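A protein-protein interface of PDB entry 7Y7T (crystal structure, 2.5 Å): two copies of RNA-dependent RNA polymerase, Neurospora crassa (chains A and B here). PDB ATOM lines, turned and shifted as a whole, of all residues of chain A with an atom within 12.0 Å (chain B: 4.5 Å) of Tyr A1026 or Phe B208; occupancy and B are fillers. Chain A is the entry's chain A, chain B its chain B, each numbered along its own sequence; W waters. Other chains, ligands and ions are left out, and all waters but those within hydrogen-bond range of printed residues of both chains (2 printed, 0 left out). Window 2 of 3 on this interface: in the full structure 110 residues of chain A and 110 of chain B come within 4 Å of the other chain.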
ATOM      1  N   PHE A1020      12.669   1.942 -11.473  1.00  0.00           N
ATOM      2  CA  PHE A1020      13.330   1.277 -10.357  1.00  0.00           C
ATOM      3  C   PHE A1020      13.835   2.312  -9.356  1.00  0.00           C
ATOM      4  O   PHE A1020      14.628   3.190  -9.708  1.00  0.00           O
ATOM      5  CB  PHE A1020      14.480   0.421 -10.883  1.00  0.00           C
ATOM      6  CG  PHE A1020      15.172  -0.396  -9.830  1.00  0.00           C
ATOM      7  CD1 PHE A1020      14.546  -1.488  -9.251  1.00  0.00           C
ATOM      8  CD2 PHE A1020      16.463  -0.084  -9.437  1.00  0.00           C
ATOM      9  CE1 PHE A1020      15.191  -2.246  -8.289  1.00  0.00           C
ATOM     10  CE2 PHE A1020      17.112  -0.837  -8.478  1.00  0.00           C
ATOM     11  CZ  PHE A1020      16.476  -1.919  -7.904  1.00  0.00           C
ATOM     12  N   THR A1021      13.367   2.214  -8.109  1.00  0.00           N
ATOM     13  CA  THR A1021      13.822   3.090  -7.034  1.00  0.00           C
ATOM     14  C   THR A1021      14.487   2.324  -5.899  1.00  0.00           C
ATOM     15  O   THR A1021      14.777   2.916  -4.852  1.00  0.00           O
ATOM     16  CB  THR A1021      12.661   3.919  -6.476  1.00  0.00           C
ATOM     17  OG1 THR A1021      11.524   3.073  -6.262  1.00  0.00           O
ATOM     18  CG2 THR A1021      12.294   5.035  -7.435  1.00  0.00           C
ATOM     19  N   GLY A1022      14.733   1.039  -6.071  1.00  0.00           N
ATOM     20  CA  GLY A1022      15.339   0.217  -5.040  1.00  0.00           C
ATOM     21  C   GLY A1022      14.698  -1.156  -4.997  1.00  0.00           C
ATOM     22  O   GLY A1022      13.613  -1.389  -5.530  1.00  0.00           O
ATOM     23  N   ASN A1023      15.388  -2.088  -4.341  1.00  0.00           N
ATOM     24  CA  ASN A1023      14.909  -3.461  -4.246  1.00  0.00           C
ATOM     25  C   ASN A1023      14.022  -3.708  -3.035  1.00  0.00           C
ATOM     26  O   ASN A1023      13.230  -4.657  -3.052  1.00  0.00           O
ATOM     27  CB  ASN A1023      16.087  -4.439  -4.212  1.00  0.00           C
ATOM     28  CG  ASN A1023      16.652  -4.713  -5.589  1.00  0.00           C
ATOM     29  OD1 ASN A1023      17.781  -4.332  -5.898  1.00  0.00           O
ATOM     30  ND2 ASN A1023      15.864  -5.371  -6.432  1.00  0.00           N
ATOM     31  N   GLY A1024      14.134  -2.893  -1.992  1.00  0.00           N
ATOM     32  CA  GLY A1024      13.327  -3.038  -0.803  1.00  0.00           C
ATOM     33  C   GLY A1024      12.709  -1.714  -0.399  1.00  0.00           C
ATOM     34  O   GLY A1024      12.389  -0.865  -1.234  1.00  0.00           O
ATOM     35  N   ASP A1025      12.536  -1.552   0.911  1.00  0.00           N
ATOM     36  CA  ASP A1025      12.057  -0.306   1.495  1.00  0.00           C
ATOM     37  C   ASP A1025      13.123   0.396   2.321  1.00  0.00           C
ATOM     38  O   ASP A1025      13.321   1.607   2.174  1.00  0.00           O
ATOM     39  CB  ASP A1025      10.816  -0.566   2.360  1.00  0.00           C
ATOM     40  CG  ASP A1025       9.665  -1.151   1.568  1.00  0.00           C
ATOM     41  OD1 ASP A1025       9.615  -0.932   0.339  1.00  0.00           O
ATOM     42  OD2 ASP A1025       8.811  -1.830   2.176  1.00  0.00           O
ATOM     43  N   TYR A1026      13.817  -0.338   3.188  1.00  0.00           N
ATOM     44  CA  TYR A1026      14.879   0.225   4.016  1.00  0.00           C
ATOM     45  C   TYR A1026      15.940   0.904   3.155  1.00  0.00           C
ATOM     46  O   TYR A1026      16.458   1.966   3.500  1.00  0.00           O
ATOM     47  CB  TYR A1026      15.538  -0.856   4.878  1.00  0.00           C
ATOM     48  CG  TYR A1026      14.590  -1.796   5.593  1.00  0.00           C
ATOM     49  CD1 TYR A1026      13.412  -1.335   6.168  1.00  0.00           C
ATOM     50  CD2 TYR A1026      14.889  -3.148   5.710  1.00  0.00           C
ATOM     51  CE1 TYR A1026      12.553  -2.198   6.827  1.00  0.00           C
ATOM     52  CE2 TYR A1026      14.039  -4.016   6.365  1.00  0.00           C
ATOM     53  CZ  TYR A1026      12.874  -3.538   6.923  1.00  0.00           C
ATOM     54  OH  TYR A1026      12.025  -4.402   7.577  1.00  0.00           O
ATOM     55  OXT TYR A1026      16.304   0.406   2.090  1.00  0.00           O
ATOM     56  N   ALA B 206      15.649 -12.076  17.849  1.00  0.00           N
ATOM     57  CA  ALA B 206      15.076 -10.964  17.104  1.00  0.00           C
ATOM     58  C   ALA B 206      15.880  -9.691  17.331  1.00  0.00           C
ATOM     59  O   ALA B 206      16.270  -9.378  18.461  1.00  0.00           O
ATOM     60  CB  ALA B 206      13.621 -10.739  17.512  1.00  0.00           C
ATOM     61  N   PHE B 207      16.119  -8.949  16.247  1.00  0.00           N
ATOM     62  CA  PHE B 207      16.867  -7.704  16.334  1.00  0.00           C
ATOM     63  C   PHE B 207      16.209  -6.520  15.639  1.00  0.00           C
ATOM     64  O   PHE B 207      16.623  -5.383  15.891  1.00  0.00           O
ATOM     65  CB  PHE B 207      18.293  -7.891  15.783  1.00  0.00           C
ATOM     66  CG  PHE B 207      18.363  -8.091  14.294  1.00  0.00           C
ATOM     67  CD1 PHE B 207      18.256  -9.359  13.746  1.00  0.00           C
ATOM     68  CD2 PHE B 207      18.587  -7.017  13.444  1.00  0.00           C
ATOM     69  CE1 PHE B 207      18.337  -9.550  12.380  1.00  0.00           C
ATOM     70  CE2 PHE B 207      18.669  -7.201  12.075  1.00  0.00           C
ATOM     71  CZ  PHE B 207      18.545  -8.471  11.543  1.00  0.00           C
ATOM     72  N   PHE B 208      15.200  -6.734  14.799  1.00  0.00           N
ATOM     73  CA  PHE B 208      14.541  -5.625  14.125  1.00  0.00           C
ATOM     74  C   PHE B 208      13.097  -5.990  13.816  1.00  0.00           C
ATOM     75  O   PHE B 208      12.760  -7.165  13.649  1.00  0.00           O
ATOM     76  CB  PHE B 208      15.265  -5.239  12.830  1.00  0.00           C
ATOM     77  CG  PHE B 208      14.779  -3.954  12.230  1.00  0.00           C
ATOM     78  CD1 PHE B 208      15.035  -2.745  12.854  1.00  0.00           C
ATOM     79  CD2 PHE B 208      14.050  -3.956  11.053  1.00  0.00           C
ATOM     80  CE1 PHE B 208      14.584  -1.560  12.310  1.00  0.00           C
ATOM     81  CE2 PHE B 208      13.594  -2.775  10.503  1.00  0.00           C
ATOM     82  CZ  PHE B 208      13.861  -1.576  11.133  1.00  0.00           C
ATOM     83  N   ALA B 209      12.250  -4.965  13.736  1.00  0.00           N
ATOM     84  CA  ALA B 209      10.871  -5.126  13.305  1.00  0.00           C
ATOM     85  C   ALA B 209      10.403  -3.833  12.657  1.00  0.00           C
ATOM     86  O   ALA B 209      10.774  -2.741  13.100  1.00  0.00           O
ATOM     87  CB  ALA B 209       9.946  -5.497  14.470  1.00  0.00           C
ATOM     88  N   LYS B 210       9.600  -3.963  11.605  1.00  0.00           N
ATOM     89  CA  LYS B 210       8.987  -2.812  10.958  1.00  0.00           C
ATOM     90  C   LYS B 210       7.748  -3.271  10.203  1.00  0.00           C
ATOM     91  O   LYS B 210       7.683  -4.406   9.721  1.00  0.00           O
ATOM     92  CB  LYS B 210       9.958  -2.098  10.006  1.00  0.00           C
ATOM     93  CG  LYS B 210       9.399  -0.801   9.442  1.00  0.00           C
ATOM     94  CD  LYS B 210      10.422   0.019   8.679  1.00  0.00           C
ATOM     95  CE  LYS B 210       9.769   1.295   8.162  1.00  0.00           C
ATOM     96  NZ  LYS B 210      10.727   2.223   7.505  1.00  0.00           N
ATOM     97  N   ARG B 235       7.035  -7.026   9.737  1.00  0.00           N
ATOM     98  CA  ARG B 235       8.159  -7.878   9.374  1.00  0.00           C
ATOM     99  C   ARG B 235       9.164  -7.876  10.517  1.00  0.00           C
ATOM    100  O   ARG B 235       9.647  -6.813  10.922  1.00  0.00           O
ATOM    101  CB  ARG B 235       8.817  -7.402   8.080  1.00  0.00           C
ATOM    102  CG  ARG B 235       9.883  -8.350   7.557  1.00  0.00           C
ATOM    103  CD  ARG B 235      10.510  -7.835   6.273  1.00  0.00           C
ATOM    104  NE  ARG B 235       9.603  -7.948   5.138  1.00  0.00           N
ATOM    105  CZ  ARG B 235       8.931  -6.933   4.613  1.00  0.00           C
ATOM    106  NH1 ARG B 235       9.038  -5.708   5.101  1.00  0.00           N
ATOM    107  NH2 ARG B 235       8.130  -7.151   3.574  1.00  0.00           N
ATOM    108  N   VAL B 236       9.470  -9.060  11.036  1.00  0.00           N
ATOM    109  CA  VAL B 236      10.425  -9.233  12.123  1.00  0.00           C
ATOM    110  C   VAL B 236      11.640  -9.973  11.583  1.00  0.00           C
ATOM    111  O   VAL B 236      11.509 -10.913  10.792  1.00  0.00           O
ATOM    112  CB  VAL B 236       9.795  -9.986  13.310  1.00  0.00           C
ATOM    113  CG1 VAL B 236      10.788 -10.105  14.453  1.00  0.00           C
ATOM    114  CG2 VAL B 236       8.530  -9.277  13.772  1.00  0.00           C
ATOM    115  N   HIS B 237      12.824  -9.542  12.009  1.00  0.00           N
ATOM    116  CA  HIS B 237      14.084 -10.102  11.544  1.00  0.00           C
ATOM    117  C   HIS B 237      14.787 -10.822  12.685  1.00  0.00           C
ATOM    118  O   HIS B 237      14.784 -10.352  13.827  1.00  0.00           O
ATOM    119  CB  HIS B 237      14.988  -9.006  10.977  1.00  0.00           C
ATOM    120  CG  HIS B 237      14.439  -8.352   9.748  1.00  0.00           C
ATOM    121  ND1 HIS B 237      14.811  -8.729   8.476  1.00  0.00           N
ATOM    122  CD2 HIS B 237      13.538  -7.354   9.596  1.00  0.00           C
ATOM    123  CE1 HIS B 237      14.167  -7.987   7.593  1.00  0.00           C
ATOM    124  NE2 HIS B 237      13.387  -7.145   8.247  1.00  0.00           N
ATOM    125  N   PHE B 293      17.808   2.288  17.069  1.00  0.00           N
ATOM    126  CA  PHE B 293      17.185   1.088  16.521  1.00  0.00           C
ATOM    127  C   PHE B 293      16.770   1.293  15.069  1.00  0.00           C
ATOM    128  O   PHE B 293      16.858   0.369  14.252  1.00  0.00           O
ATOM    129  CB  PHE B 293      15.985   0.710  17.397  1.00  0.00           C
ATOM    130  CG  PHE B 293      15.184  -0.461  16.894  1.00  0.00           C
ATOM    131  CD1 PHE B 293      15.470  -1.747  17.321  1.00  0.00           C
ATOM    132  CD2 PHE B 293      14.102  -0.268  16.048  1.00  0.00           C
ATOM    133  CE1 PHE B 293      14.720  -2.822  16.882  1.00  0.00           C
ATOM    134  CE2 PHE B 293      13.348  -1.337  15.604  1.00  0.00           C
ATOM    135  CZ  PHE B 293      13.656  -2.617  16.023  1.00  0.00           C
ATOM    136  N   ILE B 296      19.200   0.548  12.173  1.00  0.00           N
ATOM    137  CA  ILE B 296      19.395  -0.831  11.742  1.00  0.00           C
ATOM    138  C   ILE B 296      18.851  -1.046  10.335  1.00  0.00           C
ATOM    139  O   ILE B 296      19.257  -1.990   9.650  1.00  0.00           O
ATOM    140  CB  ILE B 296      18.753  -1.799  12.765  1.00  0.00           C
ATOM    141  CG1 ILE B 296      19.367  -1.591  14.150  1.00  0.00           C
ATOM    142  CG2 ILE B 296      18.918  -3.254  12.347  1.00  0.00           C
ATOM    143  CD1 ILE B 296      18.679  -2.377  15.251  1.00  0.00           C
ATOM    144  N   GLN B 297      17.948  -0.173   9.877  1.00  0.00           N
ATOM    145  CA  GLN B 297      17.480  -0.247   8.495  1.00  0.00           C
ATOM    146  C   GLN B 297      18.638  -0.133   7.513  1.00  0.00           C
ATOM    147  O   GLN B 297      18.650  -0.806   6.476  1.00  0.00           O
ATOM    148  CB  GLN B 297      16.462   0.857   8.218  1.00  0.00           C
ATOM    149  CG  GLN B 297      15.048   0.544   8.652  1.00  0.00           C
ATOM    150  CD  GLN B 297      14.142   1.757   8.562  1.00  0.00           C
ATOM    151  OE1 GLN B 297      13.980   2.341   7.491  1.00  0.00           O
ATOM    152  NE2 GLN B 297      13.560   2.151   9.691  1.00  0.00           N
ATOM    153  N   LEU B 300      20.131  -3.447   6.932  1.00  0.00           N
ATOM    154  CA  LEU B 300      19.247  -4.372   6.238  1.00  0.00           C
ATOM    155  C   LEU B 300      18.914  -3.923   4.823  1.00  0.00           C
ATOM    156  O   LEU B 300      18.347  -4.710   4.057  1.00  0.00           O
ATOM    157  CB  LEU B 300      17.949  -4.545   7.034  1.00  0.00           C
ATOM    158  CG  LEU B 300      18.076  -5.294   8.361  1.00  0.00           C
ATOM    159  CD1 LEU B 300      16.716  -5.456   9.017  1.00  0.00           C
ATOM    160  CD2 LEU B 300      18.737  -6.648   8.142  1.00  0.00           C
ATOM    161  N   SER B 301      19.254  -2.686   4.465  1.00  0.00           N
ATOM    162  CA  SER B 301      18.889  -2.124   3.169  1.00  0.00           C
ATOM    163  C   SER B 301      19.485  -2.946   2.033  1.00  0.00           C
ATOM    164  O   SER B 301      20.705  -3.121   1.953  1.00  0.00           O
ATOM    165  CB  SER B 301      19.362  -0.673   3.088  1.00  0.00           C
ATOM    166  OG  SER B 301      18.894  -0.043   1.911  1.00  0.00           O
ATOM    167  N   ARG B 362      24.337   4.045   0.387  1.00  0.00           N
ATOM    168  CA  ARG B 362      24.804   4.091   1.763  1.00  0.00           C
ATOM    169  C   ARG B 362      26.306   3.856   1.772  1.00  0.00           C
ATOM    170  O   ARG B 362      26.872   3.285   0.836  1.00  0.00           O
ATOM    171  CB  ARG B 362      24.097   3.053   2.648  1.00  0.00           C
ATOM    172  CG  ARG B 362      22.620   3.322   2.878  1.00  0.00           C
ATOM    173  CD  ARG B 362      21.765   2.642   1.824  1.00  0.00           C
ATOM    174  NE  ARG B 362      20.342   2.748   2.121  1.00  0.00           N
ATOM    175  CZ  ARG B 362      19.558   3.719   1.674  1.00  0.00           C
ATOM    176  NH1 ARG B 362      20.030   4.700   0.922  1.00  0.00           N
ATOM    177  NH2 ARG B 362      18.266   3.704   1.986  1.00  0.00           N
ATOM    178  N   ARG B 407      21.598   1.802  -3.685  1.00  0.00           N
ATOM    179  CA  ARG B 407      20.204   1.382  -3.690  1.00  0.00           C
ATOM    180  C   ARG B 407      19.577   1.527  -5.073  1.00  0.00           C
ATOM    181  O   ARG B 407      18.871   0.620  -5.527  1.00  0.00           O
ATOM    182  CB  ARG B 407      19.414   2.186  -2.653  1.00  0.00           C
ATOM    183  CG  ARG B 407      17.905   2.111  -2.796  1.00  0.00           C
ATOM    184  CD  ARG B 407      17.226   2.358  -1.455  1.00  0.00           C
ATOM    185  NE  ARG B 407      15.774   2.413  -1.574  1.00  0.00           N
ATOM    186  CZ  ARG B 407      14.978   1.352  -1.541  1.00  0.00           C
ATOM    187  NH1 ARG B 407      13.668   1.465  -1.697  1.00  0.00           N
ATOM    188  NH2 ARG B 407      15.507   0.148  -1.343  1.00  0.00           N
ATOM    189  N   PHE B 697      10.152  -2.539  20.007  1.00  0.00           N
ATOM    190  CA  PHE B 697       9.179  -3.445  19.356  1.00  0.00           C
ATOM    191  C   PHE B 697       7.772  -3.005  19.752  1.00  0.00           C
ATOM    192  O   PHE B 697       6.870  -3.091  18.924  1.00  0.00           O
ATOM    193  CB  PHE B 697       9.456  -4.897  19.738  1.00  0.00           C
ATOM    194  CG  PHE B 697      10.256  -5.704  18.747  1.00  0.00           C
ATOM    195  CD1 PHE B 697      11.439  -5.218  18.219  1.00  0.00           C
ATOM    196  CD2 PHE B 697       9.833  -6.964  18.361  1.00  0.00           C
ATOM    197  CE1 PHE B 697      12.177  -5.970  17.323  1.00  0.00           C
ATOM    198  CE2 PHE B 697      10.571  -7.715  17.464  1.00  0.00           C
ATOM    199  CZ  PHE B 697      11.743  -7.218  16.948  1.00  0.00           C
HETATM  200  O   HOH W   1      17.781  -1.683  -4.563  1.00  0.00           O
HETATM  201  O   HOH W   2      15.700   5.137   2.240  1.00  0.00           O
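A ring nitrogen (NE2) of His B237 lies within hydrogen-bond range of the side-chain hydroxyl (OH) of Tyr A1026 (3.1 Å). The side-chain hydroxyl (OG) of Ser B301 lies within hydrogen-bond range of the chain-end carboxylate (OXT) of Tyr A1026 (2.6 Å). The guanidinium group (NE) of Arg B407 lies within hydrogen-bond range of the backbone carbonyl oxygen (O) of Thr A1021, 3.5 Å away. The backbone carbonyl oxygen of Gly A1024 sits at hydrogen-bond distance from the guanidinium group of Arg B407 (2.7 Å). NH2 of Arg B407 is in salt-bridge range of OXT of Tyr A1026, at 3.5 Å. O of Tyr A1026 is in salt-bridge range of NH2 of Arg B362, 2.9 Å away.
The side-chain amino group of Lys B210 lies within hydrogen-bond range of the side-chain amide oxygen of Gln B297. The backbone NH (N) of Phe B207 lies within hydrogen-bond range of the backbone carbonyl oxygen (O) of His B237 (3.1 Å). NE of Arg B362 lies within hydrogen-bond range of OG of Ser B301, at 3.2 Å. The backbone carbonyl oxygen (O) of Phe B208 lies within hydrogen-bond range of the backbone NH (N) of His B237. O of Lys B210 is in hydrogen-bond range of N of Arg B235 (2.7 Å).
Among the printed residues, pairs that only touch across the chains: Tyr A1026 with Gln B297, Gly A1022 with Arg B407, Tyr A1026 with Lys B210, Tyr A1026 with Leu B300, Tyr A1026 with Phe B208, Phe A1020 with Arg B407, Asn A1023 with Arg B407, Asp A1025 with Arg B407 and Tyr A1026 with Arg B235.
Of chain B, only Phe B208 (3.7 Å), Lys B210 (3.6 Å), Arg B235 (3.97 Å), His B237 (3.1 Å), Gln B297 (3.5 Å), Leu B300 (3.6 Å), Ser B301 (2.6 Å), Arg B362 (2.9 Å) and Arg B407 (3.5 Å) come within 4 Å of Tyr A1026. Of chain A, only Tyr A1026 comes within 4 Å of Phe B208. No residue of chain A comes within 4 Å of Ala B206. No residue of chain A comes within 4 Å of Ala B209. Lys B210 touches just one residue of chain A: Tyr A1026 (3.6 Å). Arg B235 touches just one residue of chain A: Tyr A1026 (3.97 Å). Val B236 touches none of the printed residues of chain A. No residue of chain A comes within 4 Å of Phe B293. No residue of chain A comes within 4 Å of Ile B296. Of chain A, only Tyr A1026 (3.5 Å) comes within 4 Å of Gln B297. Of the printed residues of chain B, Asn A1023 touches Arg B407 (3.7 Å). Printed residues of chain B within 4 Å of Thr A1021: Arg B407 (3.5 Å). Of the printed residues of chain A, Arg B362 touches Tyr A1026 (2.9 Å). Printed residues of chain B within 4 Å of Gly A1024: Arg B407. Phe B697 touches none of the printed residues of chain A. The nearest printed residue of chain B that does not touch Thr A1021 is Arg B362 (7.7 Å).
Of the 16 printed residues of chain B, 9 touch a printed residue of chain A. Printed residues of chain B that touch a printed residue of chain A: Phe B208, Lys B210, Arg B235, His B237, Gln B297, Leu B300, Ser B301, Arg B362 and Arg B407. Hydrophobic or aromatic side chains of chain B within 4 Å of the printed part of chain A: Phe B208, His B237 and Leu B300. Hydrophobic or aromatic side chains of chain A within 4 Å of the printed part of chain B: Phe A1020 and Tyr A1026. Along chain A the printed residues that touch a printed residue of chain B span positions 1020 to 1026.
No position is printed for both chains.
Water W1 lies within hydrogen-bond range of N of Asn A1023 (2.4 Å) and O of Arg B407 (2.7 Å). Water W2 bridges NH2 of Arg B362 (2.9 Å) and O of Tyr A1026 (3.5 Å).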
